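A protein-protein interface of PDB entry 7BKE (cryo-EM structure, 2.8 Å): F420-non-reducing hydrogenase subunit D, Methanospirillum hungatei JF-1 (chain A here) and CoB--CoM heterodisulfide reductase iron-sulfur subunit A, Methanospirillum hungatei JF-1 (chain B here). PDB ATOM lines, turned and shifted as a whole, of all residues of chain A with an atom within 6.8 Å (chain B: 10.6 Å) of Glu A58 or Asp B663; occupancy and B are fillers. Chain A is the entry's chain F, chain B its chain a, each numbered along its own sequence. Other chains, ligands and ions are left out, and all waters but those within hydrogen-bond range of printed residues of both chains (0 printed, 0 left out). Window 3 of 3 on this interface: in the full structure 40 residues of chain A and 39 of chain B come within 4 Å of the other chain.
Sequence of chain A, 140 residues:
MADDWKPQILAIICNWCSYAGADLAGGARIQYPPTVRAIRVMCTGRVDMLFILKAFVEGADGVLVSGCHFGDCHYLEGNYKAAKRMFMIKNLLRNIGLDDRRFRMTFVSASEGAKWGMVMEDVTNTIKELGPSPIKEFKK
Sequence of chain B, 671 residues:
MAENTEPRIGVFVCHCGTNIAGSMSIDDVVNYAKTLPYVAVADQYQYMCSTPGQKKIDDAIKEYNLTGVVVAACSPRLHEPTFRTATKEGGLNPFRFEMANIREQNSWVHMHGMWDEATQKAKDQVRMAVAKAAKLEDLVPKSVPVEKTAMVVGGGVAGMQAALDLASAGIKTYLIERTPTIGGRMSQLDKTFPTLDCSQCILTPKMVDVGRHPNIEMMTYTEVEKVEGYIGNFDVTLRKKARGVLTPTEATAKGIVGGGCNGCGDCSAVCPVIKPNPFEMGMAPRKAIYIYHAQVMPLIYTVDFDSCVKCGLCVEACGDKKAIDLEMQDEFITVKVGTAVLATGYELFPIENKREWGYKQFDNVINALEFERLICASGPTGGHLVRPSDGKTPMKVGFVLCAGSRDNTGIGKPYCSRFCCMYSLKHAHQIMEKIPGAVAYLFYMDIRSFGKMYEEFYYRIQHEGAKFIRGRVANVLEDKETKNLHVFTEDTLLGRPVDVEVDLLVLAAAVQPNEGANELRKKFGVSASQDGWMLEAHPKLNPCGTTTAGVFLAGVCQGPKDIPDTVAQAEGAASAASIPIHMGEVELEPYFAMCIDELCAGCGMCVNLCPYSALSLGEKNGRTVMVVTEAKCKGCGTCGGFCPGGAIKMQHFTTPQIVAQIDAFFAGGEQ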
ATOM      1  N   GLN A   8     -21.017   1.778   5.042  1.00  0.00           N
ATOM      2  CA  GLN A   8     -21.360   2.764   6.058  1.00  0.00           C
ATOM      3  C   GLN A   8     -20.417   2.556   7.229  1.00  0.00           C
ATOM      4  O   GLN A   8     -20.669   1.713   8.090  1.00  0.00           O
ATOM      5  CB  GLN A   8     -22.805   2.616   6.497  1.00  0.00           C
ATOM      6  CG  GLN A   8     -23.809   2.902   5.421  1.00  0.00           C
ATOM      7  CD  GLN A   8     -25.197   3.094   5.977  1.00  0.00           C
ATOM      8  OE1 GLN A   8     -25.962   2.143   6.109  1.00  0.00           O
ATOM      9  NE2 GLN A   8     -25.525   4.330   6.327  1.00  0.00           N
ATOM     10  N   LEU A  10     -18.449   4.203  10.533  1.00  0.00           N
ATOM     11  CA  LEU A  10     -18.584   5.249  11.532  1.00  0.00           C
ATOM     12  C   LEU A  10     -17.329   5.273  12.381  1.00  0.00           C
ATOM     13  O   LEU A  10     -16.886   4.230  12.858  1.00  0.00           O
ATOM     14  CB  LEU A  10     -19.818   5.005  12.400  1.00  0.00           C
ATOM     15  CG  LEU A  10     -20.101   5.970  13.547  1.00  0.00           C
ATOM     16  CD1 LEU A  10     -21.567   6.294  13.587  1.00  0.00           C
ATOM     17  CD2 LEU A  10     -19.679   5.362  14.867  1.00  0.00           C
ATOM     18  N   LEU A  53     -22.240  -0.953  19.999  1.00  0.00           N
ATOM     19  CA  LEU A  53     -23.277  -1.935  19.723  1.00  0.00           C
ATOM     20  C   LEU A  53     -24.484  -1.290  19.062  1.00  0.00           C
ATOM     21  O   LEU A  53     -25.110  -1.891  18.185  1.00  0.00           O
ATOM     22  CB  LEU A  53     -23.671  -2.651  21.007  1.00  0.00           C
ATOM     23  CG  LEU A  53     -22.504  -3.403  21.636  1.00  0.00           C
ATOM     24  CD1 LEU A  53     -22.958  -4.154  22.856  1.00  0.00           C
ATOM     25  CD2 LEU A  53     -21.883  -4.341  20.635  1.00  0.00           C
ATOM     26  N   LYS A  54     -24.829  -0.070  19.467  1.00  0.00           N
ATOM     27  CA  LYS A  54     -25.910   0.658  18.824  1.00  0.00           C
ATOM     28  C   LYS A  54     -25.587   0.935  17.368  1.00  0.00           C
ATOM     29  O   LYS A  54     -26.452   0.798  16.502  1.00  0.00           O
ATOM     30  CB  LYS A  54     -26.169   1.957  19.580  1.00  0.00           C
ATOM     31  CG  LYS A  54     -27.231   2.841  18.985  1.00  0.00           C
ATOM     32  CD  LYS A  54     -28.594   2.236  19.150  1.00  0.00           C
ATOM     33  CE  LYS A  54     -29.660   3.294  19.102  1.00  0.00           C
ATOM     34  NZ  LYS A  54     -30.957   2.715  18.694  1.00  0.00           N
ATOM     35  N   ALA A  55     -24.349   1.325  17.074  1.00  0.00           N
ATOM     36  CA  ALA A  55     -23.953   1.524  15.685  1.00  0.00           C
ATOM     37  C   ALA A  55     -24.111   0.241  14.884  1.00  0.00           C
ATOM     38  O   ALA A  55     -24.703   0.234  13.795  1.00  0.00           O
ATOM     39  CB  ALA A  55     -22.513   2.015  15.624  1.00  0.00           C
ATOM     40  N   PHE A  56     -23.603  -0.866  15.419  1.00  0.00           N
ATOM     41  CA  PHE A  56     -23.642  -2.124  14.685  1.00  0.00           C
ATOM     42  C   PHE A  56     -25.058  -2.642  14.511  1.00  0.00           C
ATOM     43  O   PHE A  56     -25.338  -3.338  13.533  1.00  0.00           O
ATOM     44  CB  PHE A  56     -22.792  -3.170  15.386  1.00  0.00           C
ATOM     45  CG  PHE A  56     -21.403  -3.218  14.894  1.00  0.00           C
ATOM     46  CD1 PHE A  56     -21.147  -3.359  13.551  1.00  0.00           C
ATOM     47  CD2 PHE A  56     -20.350  -3.101  15.762  1.00  0.00           C
ATOM     48  CE1 PHE A  56     -19.874  -3.391  13.094  1.00  0.00           C
ATOM     49  CE2 PHE A  56     -19.074  -3.133  15.306  1.00  0.00           C
ATOM     50  CZ  PHE A  56     -18.833  -3.279  13.974  1.00  0.00           C
ATOM     51  N   VAL A  57     -25.956  -2.343  15.448  1.00  0.00           N
ATOM     52  CA  VAL A  57     -27.329  -2.803  15.294  1.00  0.00           C
ATOM     53  C   VAL A  57     -28.146  -1.853  14.431  1.00  0.00           C
ATOM     54  O   VAL A  57     -29.141  -2.278  13.840  1.00  0.00           O
ATOM     55  CB  VAL A  57     -28.014  -3.008  16.656  1.00  0.00           C
ATOM     56  CG1 VAL A  57     -28.330  -1.689  17.300  1.00  0.00           C
ATOM     57  CG2 VAL A  57     -29.269  -3.846  16.503  1.00  0.00           C
ATOM     58  N   GLU A  58     -27.775  -0.578  14.334  1.00  0.00           N
ATOM     59  CA  GLU A  58     -28.400   0.268  13.325  1.00  0.00           C
ATOM     60  C   GLU A  58     -27.921  -0.056  11.928  1.00  0.00           C
ATOM     61  O   GLU A  58     -28.618   0.269  10.963  1.00  0.00           O
ATOM     62  CB  GLU A  58     -28.165   1.754  13.589  1.00  0.00           C
ATOM     63  CG  GLU A  58     -28.589   2.223  14.943  1.00  0.00           C
ATOM     64  CD  GLU A  58     -30.067   2.511  14.988  1.00  0.00           C
ATOM     65  OE1 GLU A  58     -30.779   2.127  14.035  1.00  0.00           O
ATOM     66  OE2 GLU A  58     -30.532   3.096  15.987  1.00  0.00           O
ATOM     67  N   GLY A  59     -26.750  -0.657  11.792  1.00  0.00           N
ATOM     68  CA  GLY A  59     -26.373  -1.139  10.488  1.00  0.00           C
ATOM     69  C   GLY A  59     -25.021  -0.678  10.006  1.00  0.00           C
ATOM     70  O   GLY A  59     -24.767  -0.682   8.804  1.00  0.00           O
ATOM     71  N   ALA A  60     -24.150  -0.269  10.915  1.00  0.00           N
ATOM     72  CA  ALA A  60     -22.797   0.076  10.519  1.00  0.00           C
ATOM     73  C   ALA A  60     -22.119  -1.131   9.904  1.00  0.00           C
ATOM     74  O   ALA A  60     -21.970  -2.168  10.555  1.00  0.00           O
ATOM     75  CB  ALA A  60     -21.998   0.572  11.717  1.00  0.00           C
ATOM     76  N   ILE A 135     -26.919  -7.828   9.811  1.00  0.00           N
ATOM     77  CA  ILE A 135     -28.025  -7.403  10.661  1.00  0.00           C
ATOM     78  C   ILE A 135     -29.148  -6.807   9.821  1.00  0.00           C
ATOM     79  O   ILE A 135     -30.337  -7.011  10.103  1.00  0.00           O
ATOM     80  CB  ILE A 135     -27.518  -6.403  11.713  1.00  0.00           C
ATOM     81  CG1 ILE A 135     -26.363  -7.009  12.498  1.00  0.00           C
ATOM     82  CG2 ILE A 135     -28.635  -6.017  12.650  1.00  0.00           C
ATOM     83  CD1 ILE A 135     -26.774  -8.068  13.447  1.00  0.00           C
ATOM     84  N   LYS A 136     -28.784  -6.076   8.767  1.00  0.00           N
ATOM     85  CA  LYS A 136     -29.767  -5.345   7.979  1.00  0.00           C
ATOM     86  C   LYS A 136     -30.770  -6.279   7.313  1.00  0.00           C
ATOM     87  O   LYS A 136     -31.910  -5.887   7.045  1.00  0.00           O
ATOM     88  CB  LYS A 136     -29.053  -4.490   6.938  1.00  0.00           C
ATOM     89  CG  LYS A 136     -28.006  -3.577   7.535  1.00  0.00           C
ATOM     90  CD  LYS A 136     -27.599  -2.490   6.569  1.00  0.00           C
ATOM     91  CE  LYS A 136     -26.451  -2.935   5.699  1.00  0.00           C
ATOM     92  NZ  LYS A 136     -25.191  -3.020   6.475  1.00  0.00           N
ATOM     93  N   LYS A 139     -32.822  -8.570  10.514  1.00  0.00           N
ATOM     94  CA  LYS A 139     -33.940  -7.914  11.184  1.00  0.00           C
ATOM     95  C   LYS A 139     -35.274  -8.266  10.537  1.00  0.00           C
ATOM     96  O   LYS A 139     -36.111  -8.930  11.154  1.00  0.00           O
ATOM     97  CB  LYS A 139     -33.785  -6.397  11.163  1.00  0.00           C
ATOM     98  CG  LYS A 139     -32.751  -5.829  12.093  1.00  0.00           C
ATOM     99  CD  LYS A 139     -32.700  -4.332  11.889  1.00  0.00           C
ATOM    100  CE  LYS A 139     -31.414  -3.746  12.391  1.00  0.00           C
ATOM    101  NZ  LYS A 139     -31.190  -2.392  11.824  1.00  0.00           N
ATOM    102  N   TYR B  32     -30.582  20.666   1.365  1.00  0.00           N
ATOM    103  CA  TYR B  32     -30.767  19.525   2.249  1.00  0.00           C
ATOM    104  C   TYR B  32     -30.944  19.972   3.693  1.00  0.00           C
ATOM    105  O   TYR B  32     -31.780  19.429   4.423  1.00  0.00           O
ATOM    106  CB  TYR B  32     -29.580  18.580   2.128  1.00  0.00           C
ATOM    107  CG  TYR B  32     -29.748  17.317   2.918  1.00  0.00           C
ATOM    108  CD1 TYR B  32     -30.608  16.330   2.492  1.00  0.00           C
ATOM    109  CD2 TYR B  32     -29.046  17.114   4.091  1.00  0.00           C
ATOM    110  CE1 TYR B  32     -30.763  15.176   3.201  1.00  0.00           C
ATOM    111  CE2 TYR B  32     -29.196  15.959   4.813  1.00  0.00           C
ATOM    112  CZ  TYR B  32     -30.057  14.993   4.361  1.00  0.00           C
ATOM    113  OH  TYR B  32     -30.222  13.829   5.066  1.00  0.00           O
ATOM    114  N   LEU B  36     -34.100  19.327   6.245  1.00  0.00           N
ATOM    115  CA  LEU B  36     -33.871  18.547   7.453  1.00  0.00           C
ATOM    116  C   LEU B  36     -34.918  18.874   8.516  1.00  0.00           C
ATOM    117  O   LEU B  36     -35.495  19.963   8.514  1.00  0.00           O
ATOM    118  CB  LEU B  36     -32.477  18.827   8.013  1.00  0.00           C
ATOM    119  CG  LEU B  36     -31.333  17.980   7.479  1.00  0.00           C
ATOM    120  CD1 LEU B  36     -30.042  18.354   8.163  1.00  0.00           C
ATOM    121  CD2 LEU B  36     -31.638  16.524   7.681  1.00  0.00           C
ATOM    122  N   PRO B  37     -35.198  17.942   9.426  1.00  0.00           N
ATOM    123  CA  PRO B  37     -36.080  18.253  10.553  1.00  0.00           C
ATOM    124  C   PRO B  37     -35.401  19.146  11.579  1.00  0.00           C
ATOM    125  O   PRO B  37     -34.193  19.070  11.798  1.00  0.00           O
ATOM    126  CB  PRO B  37     -36.386  16.877  11.148  1.00  0.00           C
ATOM    127  CG  PRO B  37     -35.209  16.064  10.789  1.00  0.00           C
ATOM    128  CD  PRO B  37     -34.819  16.520   9.417  1.00  0.00           C
ATOM    129  N   ASP B 124     -24.245  14.321   5.263  1.00  0.00           N
ATOM    130  CA  ASP B 124     -24.236  13.470   6.446  1.00  0.00           C
ATOM    131  C   ASP B 124     -23.686  14.202   7.659  1.00  0.00           C
ATOM    132  O   ASP B 124     -24.239  14.098   8.758  1.00  0.00           O
ATOM    133  CB  ASP B 124     -23.426  12.207   6.176  1.00  0.00           C
ATOM    134  CG  ASP B 124     -24.048  11.335   5.112  1.00  0.00           C
ATOM    135  OD1 ASP B 124     -24.972  11.806   4.423  1.00  0.00           O
ATOM    136  OD2 ASP B 124     -23.611  10.175   4.955  1.00  0.00           O
ATOM    137  N   ARG B 127     -26.218  16.678   8.899  1.00  0.00           N
ATOM    138  CA  ARG B 127     -27.311  15.996   9.580  1.00  0.00           C
ATOM    139  C   ARG B 127     -26.920  15.587  10.993  1.00  0.00           C
ATOM    140  O   ARG B 127     -27.693  15.774  11.937  1.00  0.00           O
ATOM    141  CB  ARG B 127     -27.739  14.782   8.769  1.00  0.00           C
ATOM    142  CG  ARG B 127     -29.124  14.306   9.060  1.00  0.00           C
ATOM    143  CD  ARG B 127     -29.486  13.151   8.165  1.00  0.00           C
ATOM    144  NE  ARG B 127     -28.437  12.145   8.131  1.00  0.00           N
ATOM    145  CZ  ARG B 127     -27.845  11.730   7.022  1.00  0.00           C
ATOM    146  NH1 ARG B 127     -28.202  12.236   5.857  1.00  0.00           N
ATOM    147  NH2 ARG B 127     -26.899  10.812   7.074  1.00  0.00           N
ATOM    148  N   MET B 128     -25.725  15.030  11.161  1.00  0.00           N
ATOM    149  CA  MET B 128     -25.279  14.646  12.497  1.00  0.00           C
ATOM    150  C   MET B 128     -25.110  15.861  13.403  1.00  0.00           C
ATOM    151  O   MET B 128     -25.463  15.821  14.590  1.00  0.00           O
ATOM    152  CB  MET B 128     -23.988  13.842  12.399  1.00  0.00           C
ATOM    153  CG  MET B 128     -24.123  12.636  11.496  1.00  0.00           C
ATOM    154  SD  MET B 128     -22.605  11.758  11.133  1.00  0.00           S
ATOM    155  CE  MET B 128     -21.812  11.787  12.714  1.00  0.00           C
ATOM    156  N   ALA B 129     -24.583  16.960  12.860  1.00  0.00           N
ATOM    157  CA  ALA B 129     -24.427  18.165  13.665  1.00  0.00           C
ATOM    158  C   ALA B 129     -25.775  18.721  14.098  1.00  0.00           C
ATOM    159  O   ALA B 129     -25.938  19.133  15.250  1.00  0.00           O
ATOM    160  CB  ALA B 129     -23.637  19.214  12.893  1.00  0.00           C
ATOM    161  N   VAL B 130     -26.751  18.746  13.190  1.00  0.00           N
ATOM    162  CA  VAL B 130     -28.082  19.232  13.542  1.00  0.00           C
ATOM    163  C   VAL B 130     -28.713  18.343  14.598  1.00  0.00           C
ATOM    164  O   VAL B 130     -29.373  18.825  15.524  1.00  0.00           O
ATOM    165  CB  VAL B 130     -28.973  19.330  12.293  1.00  0.00           C
ATOM    166  CG1 VAL B 130     -30.408  19.567  12.697  1.00  0.00           C
ATOM    167  CG2 VAL B 130     -28.499  20.436  11.399  1.00  0.00           C
ATOM    168  N   ALA B 131     -28.529  17.027  14.477  1.00  0.00           N
ATOM    169  CA  ALA B 131     -29.092  16.118  15.466  1.00  0.00           C
ATOM    170  C   ALA B 131     -28.505  16.354  16.848  1.00  0.00           C
ATOM    171  O   ALA B 131     -29.223  16.298  17.847  1.00  0.00           O
ATOM    172  CB  ALA B 131     -28.867  14.676  15.040  1.00  0.00           C
ATOM    173  N   LYS B 132     -27.196  16.591  16.938  1.00  0.00           N
ATOM    174  CA  LYS B 132     -26.629  16.904  18.248  1.00  0.00           C
ATOM    175  C   LYS B 132     -27.136  18.245  18.771  1.00  0.00           C
ATOM    176  O   LYS B 132     -27.495  18.366  19.951  1.00  0.00           O
ATOM    177  CB  LYS B 132     -25.107  16.910  18.190  1.00  0.00           C
ATOM    178  CG  LYS B 132     -24.456  17.231  19.519  1.00  0.00           C
ATOM    179  CD  LYS B 132     -22.956  17.164  19.422  1.00  0.00           C
ATOM    180  CE  LYS B 132     -22.277  17.722  20.656  1.00  0.00           C
ATOM    181  NZ  LYS B 132     -22.135  16.724  21.737  1.00  0.00           N
ATOM    182  N   LYS B 135     -30.361  18.704  20.589  1.00  0.00           N
ATOM    183  CA  LYS B 135     -30.398  18.160  21.932  1.00  0.00           C
ATOM    184  C   LYS B 135     -29.418  18.815  22.885  1.00  0.00           C
ATOM    185  O   LYS B 135     -29.418  18.466  24.068  1.00  0.00           O
ATOM    186  CB  LYS B 135     -30.118  16.653  21.908  1.00  0.00           C
ATOM    187  CG  LYS B 135     -31.345  15.831  21.686  1.00  0.00           C
ATOM    188  CD  LYS B 135     -31.000  14.387  21.514  1.00  0.00           C
ATOM    189  CE  LYS B 135     -32.255  13.552  21.450  1.00  0.00           C
ATOM    190  NZ  LYS B 135     -33.277  14.170  20.565  1.00  0.00           N
ATOM    191  N   THR B 655     -25.048  11.039  26.584  1.00  0.00           N
ATOM    192  CA  THR B 655     -25.399   9.841  25.805  1.00  0.00           C
ATOM    193  C   THR B 655     -26.541  10.194  24.864  1.00  0.00           C
ATOM    194  O   THR B 655     -26.405   9.880  23.691  1.00  0.00           O
ATOM    195  CB  THR B 655     -25.759   8.664  26.710  1.00  0.00           C
ATOM    196  OG1 THR B 655     -24.618   8.342  27.500  1.00  0.00           O
ATOM    197  CG2 THR B 655     -26.223   7.444  25.949  1.00  0.00           C
ATOM    198  N   PRO B 656     -27.681  10.795  25.274  1.00  0.00           N
ATOM    199  CA  PRO B 656     -28.706  11.111  24.271  1.00  0.00           C
ATOM    200  C   PRO B 656     -28.168  11.889  23.088  1.00  0.00           C
ATOM    201  O   PRO B 656     -28.581  11.628  21.955  1.00  0.00           O
ATOM    202  CB  PRO B 656     -29.724  11.923  25.072  1.00  0.00           C
ATOM    203  CG  PRO B 656     -29.570  11.460  26.429  1.00  0.00           C
ATOM    204  CD  PRO B 656     -28.133  11.165  26.623  1.00  0.00           C
ATOM    205  N   GLN B 657     -27.222  12.803  23.306  1.00  0.00           N
ATOM    206  CA  GLN B 657     -26.668  13.580  22.204  1.00  0.00           C
ATOM    207  C   GLN B 657     -25.838  12.709  21.271  1.00  0.00           C
ATOM    208  O   GLN B 657     -26.008  12.750  20.046  1.00  0.00           O
ATOM    209  CB  GLN B 657     -25.823  14.721  22.753  1.00  0.00           C
ATOM    210  CG  GLN B 657     -26.603  15.967  23.042  1.00  0.00           C
ATOM    211  CD  GLN B 657     -26.039  16.734  24.196  1.00  0.00           C
ATOM    212  OE1 GLN B 657     -24.877  16.574  24.545  1.00  0.00           O
ATOM    213  NE2 GLN B 657     -26.855  17.576  24.802  1.00  0.00           N
ATOM    214  N   ILE B 658     -24.939  11.901  21.832  1.00  0.00           N
ATOM    215  CA  ILE B 658     -24.097  11.061  20.989  1.00  0.00           C
ATOM    216  C   ILE B 658     -24.936  10.026  20.245  1.00  0.00           C
ATOM    217  O   ILE B 658     -24.708   9.751  19.060  1.00  0.00           O
ATOM    218  CB  ILE B 658     -22.990  10.415  21.830  1.00  0.00           C
ATOM    219  CG1 ILE B 658     -22.064  11.497  22.359  1.00  0.00           C
ATOM    220  CG2 ILE B 658     -22.196   9.453  21.004  1.00  0.00           C
ATOM    221  CD1 ILE B 658     -21.034  10.994  23.295  1.00  0.00           C
ATOM    222  N   VAL B 659     -25.920   9.440  20.919  1.00  0.00           N
ATOM    223  CA  VAL B 659     -26.772   8.459  20.270  1.00  0.00           C
ATOM    224  C   VAL B 659     -27.647   9.112  19.212  1.00  0.00           C
ATOM    225  O   VAL B 659     -27.958   8.492  18.195  1.00  0.00           O
ATOM    226  CB  VAL B 659     -27.594   7.713  21.335  1.00  0.00           C
ATOM    227  CG1 VAL B 659     -28.802   7.048  20.724  1.00  0.00           C
ATOM    228  CG2 VAL B 659     -26.721   6.697  22.035  1.00  0.00           C
ATOM    229  N   ALA B 660     -28.045  10.369  19.409  1.00  0.00           N
ATOM    230  CA  ALA B 660     -28.761  11.083  18.357  1.00  0.00           C
ATOM    231  C   ALA B 660     -27.875  11.293  17.143  1.00  0.00           C
ATOM    232  O   ALA B 660     -28.344  11.224  16.005  1.00  0.00           O
ATOM    233  CB  ALA B 660     -29.268  12.420  18.878  1.00  0.00           C
ATOM    234  N   GLN B 661     -26.590  11.559  17.362  1.00  0.00           N
ATOM    235  CA  GLN B 661     -25.667  11.673  16.238  1.00  0.00           C
ATOM    236  C   GLN B 661     -25.564  10.360  15.472  1.00  0.00           C
ATOM    237  O   GLN B 661     -25.604  10.343  14.234  1.00  0.00           O
ATOM    238  CB  GLN B 661     -24.296  12.108  16.734  1.00  0.00           C
ATOM    239  CG  GLN B 661     -24.135  13.592  16.819  1.00  0.00           C
ATOM    240  CD  GLN B 661     -22.783  13.978  17.319  1.00  0.00           C
ATOM    241  OE1 GLN B 661     -22.427  13.682  18.453  1.00  0.00           O
ATOM    242  NE2 GLN B 661     -22.011  14.643  16.481  1.00  0.00           N
ATOM    243  N   ILE B 662     -25.437   9.244  16.190  1.00  0.00           N
ATOM    244  CA  ILE B 662     -25.366   7.937  15.534  1.00  0.00           C
ATOM    245  C   ILE B 662     -26.646   7.662  14.745  1.00  0.00           C
ATOM    246  O   ILE B 662     -26.611   7.237  13.578  1.00  0.00           O
ATOM    247  CB  ILE B 662     -25.102   6.836  16.578  1.00  0.00           C
ATOM    248  CG1 ILE B 662     -23.652   6.881  17.027  1.00  0.00           C
ATOM    249  CG2 ILE B 662     -25.417   5.484  16.010  1.00  0.00           C
ATOM    250  CD1 ILE B 662     -23.425   6.267  18.369  1.00  0.00           C
ATOM    251  N   ASP B 663     -27.794   7.909  15.369  1.00  0.00           N
ATOM    252  CA  ASP B 663     -29.069   7.677  14.708  1.00  0.00           C
ATOM    253  C   ASP B 663     -29.209   8.531  13.459  1.00  0.00           C
ATOM    254  O   ASP B 663     -29.713   8.063  12.435  1.00  0.00           O
ATOM    255  CB  ASP B 663     -30.210   7.964  15.678  1.00  0.00           C
ATOM    256  CG  ASP B 663     -30.424   6.847  16.666  1.00  0.00           C
ATOM    257  OD1 ASP B 663     -29.905   5.745  16.416  1.00  0.00           O
ATOM    258  OD2 ASP B 663     -31.100   7.070  17.693  1.00  0.00           O
ATOM    259  N   ALA B 664     -28.779   9.791  13.528  1.00  0.00           N
ATOM    260  CA  ALA B 664     -28.853  10.664  12.365  1.00  0.00           C
ATOM    261  C   ALA B 664     -27.923  10.203  11.261  1.00  0.00           C
ATOM    262  O   ALA B 664     -28.246  10.367  10.082  1.00  0.00           O
ATOM    263  CB  ALA B 664     -28.520  12.096  12.752  1.00  0.00           C
ATOM    264  N   PHE B 665     -26.765   9.651  11.615  1.00  0.00           N
ATOM    265  CA  PHE B 665     -25.900   9.088  10.588  1.00  0.00           C
ATOM    266  C   PHE B 665     -26.602   7.965   9.849  1.00  0.00           C
ATOM    267  O   PHE B 665     -26.523   7.872   8.623  1.00  0.00           O
ATOM    268  CB  PHE B 665     -24.596   8.579  11.190  1.00  0.00           C
ATOM    269  CG  PHE B 665     -23.769   7.777  10.232  1.00  0.00           C
ATOM    270  CD1 PHE B 665     -23.523   8.238   8.952  1.00  0.00           C
ATOM    271  CD2 PHE B 665     -23.245   6.558  10.604  1.00  0.00           C
ATOM    272  CE1 PHE B 665     -22.776   7.497   8.071  1.00  0.00           C
ATOM    273  CE2 PHE B 665     -22.492   5.816   9.725  1.00  0.00           C
ATOM    274  CZ  PHE B 665     -22.257   6.287   8.462  1.00  0.00           C
ATOM    275  N   PHE B 666     -27.301   7.106  10.574  1.00  0.00           N
ATOM    276  CA  PHE B 666     -27.936   5.996   9.869  1.00  0.00           C
ATOM    277  C   PHE B 666     -29.292   6.348   9.280  1.00  0.00           C
ATOM    278  O   PHE B 666     -29.855   5.530   8.547  1.00  0.00           O
ATOM    279  CB  PHE B 666     -28.043   4.791  10.787  1.00  0.00           C
ATOM    280  CG  PHE B 666     -26.722   4.201  11.108  1.00  0.00           C
ATOM    281  CD1 PHE B 666     -26.027   3.504  10.154  1.00  0.00           C
ATOM    282  CD2 PHE B 666     -26.144   4.397  12.335  1.00  0.00           C
ATOM    283  CE1 PHE B 666     -24.798   2.988  10.432  1.00  0.00           C
ATOM    284  CE2 PHE B 666     -24.916   3.878  12.616  1.00  0.00           C
ATOM    285  CZ  PHE B 666     -24.243   3.177  11.665  1.00  0.00           C
ATOM    286  N   ALA B 667     -29.826   7.527   9.571  1.00  0.00           N
ATOM    287  CA  ALA B 667     -31.025   7.982   8.879  1.00  0.00           C
ATOM    288  C   ALA B 667     -30.742   8.163   7.391  1.00  0.00           C
ATOM    289  O   ALA B 667     -29.685   8.657   6.998  1.00  0.00           O
ATOM    290  CB  ALA B 667     -31.525   9.291   9.479  1.00  0.00           C
ATOM    291  N   GLY B 668     -31.694   7.753   6.563  1.00  0.00           N
ATOM    292  CA  GLY B 668     -31.534   7.852   5.124  1.00  0.00           C
ATOM    293  C   GLY B 668     -32.613   8.676   4.449  1.00  0.00           C
ATOM    294  O   GLY B 668     -32.929   8.462   3.277  1.00  0.00           O
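The backbone carbonyl oxygen (O) of Ala A55 is in hydrogen-bond range of the backbone NH (N) of Ala A60, 3.0 Å away. The side-chain amino group (NZ) of Lys A136 sits at hydrogen-bond distance from the backbone carbonyl oxygen (O) of Gly A59. NH2 of Arg B127 sits at hydrogen-bond distance from O of Phe B665. The side-chain carboxylate of Glu A58 is in salt-bridge range of the side-chain amino group of Lys A54 (2.8 Å).
Of the printed residues of chain B, Leu A10 touches Phe B665 (3.4 Å). Ala A55 touches one residue of chain B. No residue of chain B comes within 4 Å of Val A57. Glu A58 touches two residues of chain B. Of chain B, only Phe B666 (3.7 Å) comes within 4 Å of Gly A59. Asp B663 touches just these residues of chain A: Lys A54 and Glu A58. Printed residues of chain A within 4 Å of Phe B665: Leu A10 (3.4 Å). The nearest residue of chain B that does not touch Glu A58 is Ile B662 (4.7 Å). The nearest printed residue of chain A that does not touch Phe B665 is Gln A8 (4.2 Å).
Hydrophobic or aromatic side chains of chain A within 4 Å of the printed part of chain B: Leu A10 and Ala A60. Of the 25 printed residues of chain B, 3 touch a printed residue of chain A. Among the printed residues, 8 pairs touch across the chains. Among the printed residues, Asp or Glu carboxylates within 4 Å of a Lys or Arg side-chain nitrogen of the other chain: Lys A54 with Asp B663 (3.9 Å).
The side-chain carboxylate of Asp B663 lies within salt-bridge range of the side-chain amino group of Lys A54, 3.9 Å away. OE2 of Glu A58 lies close to OD1 of Asp B663, 2.8 Å away.
Phe B666 touches Gln A8. Leu A10 touches Phe B665. Ala A55 touches Phe B666. Phe B666 touches Glu A58. CE1 of Phe B666 touches C of Gly A59, at 3.7 Å. Ala A60 touches Phe B666.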
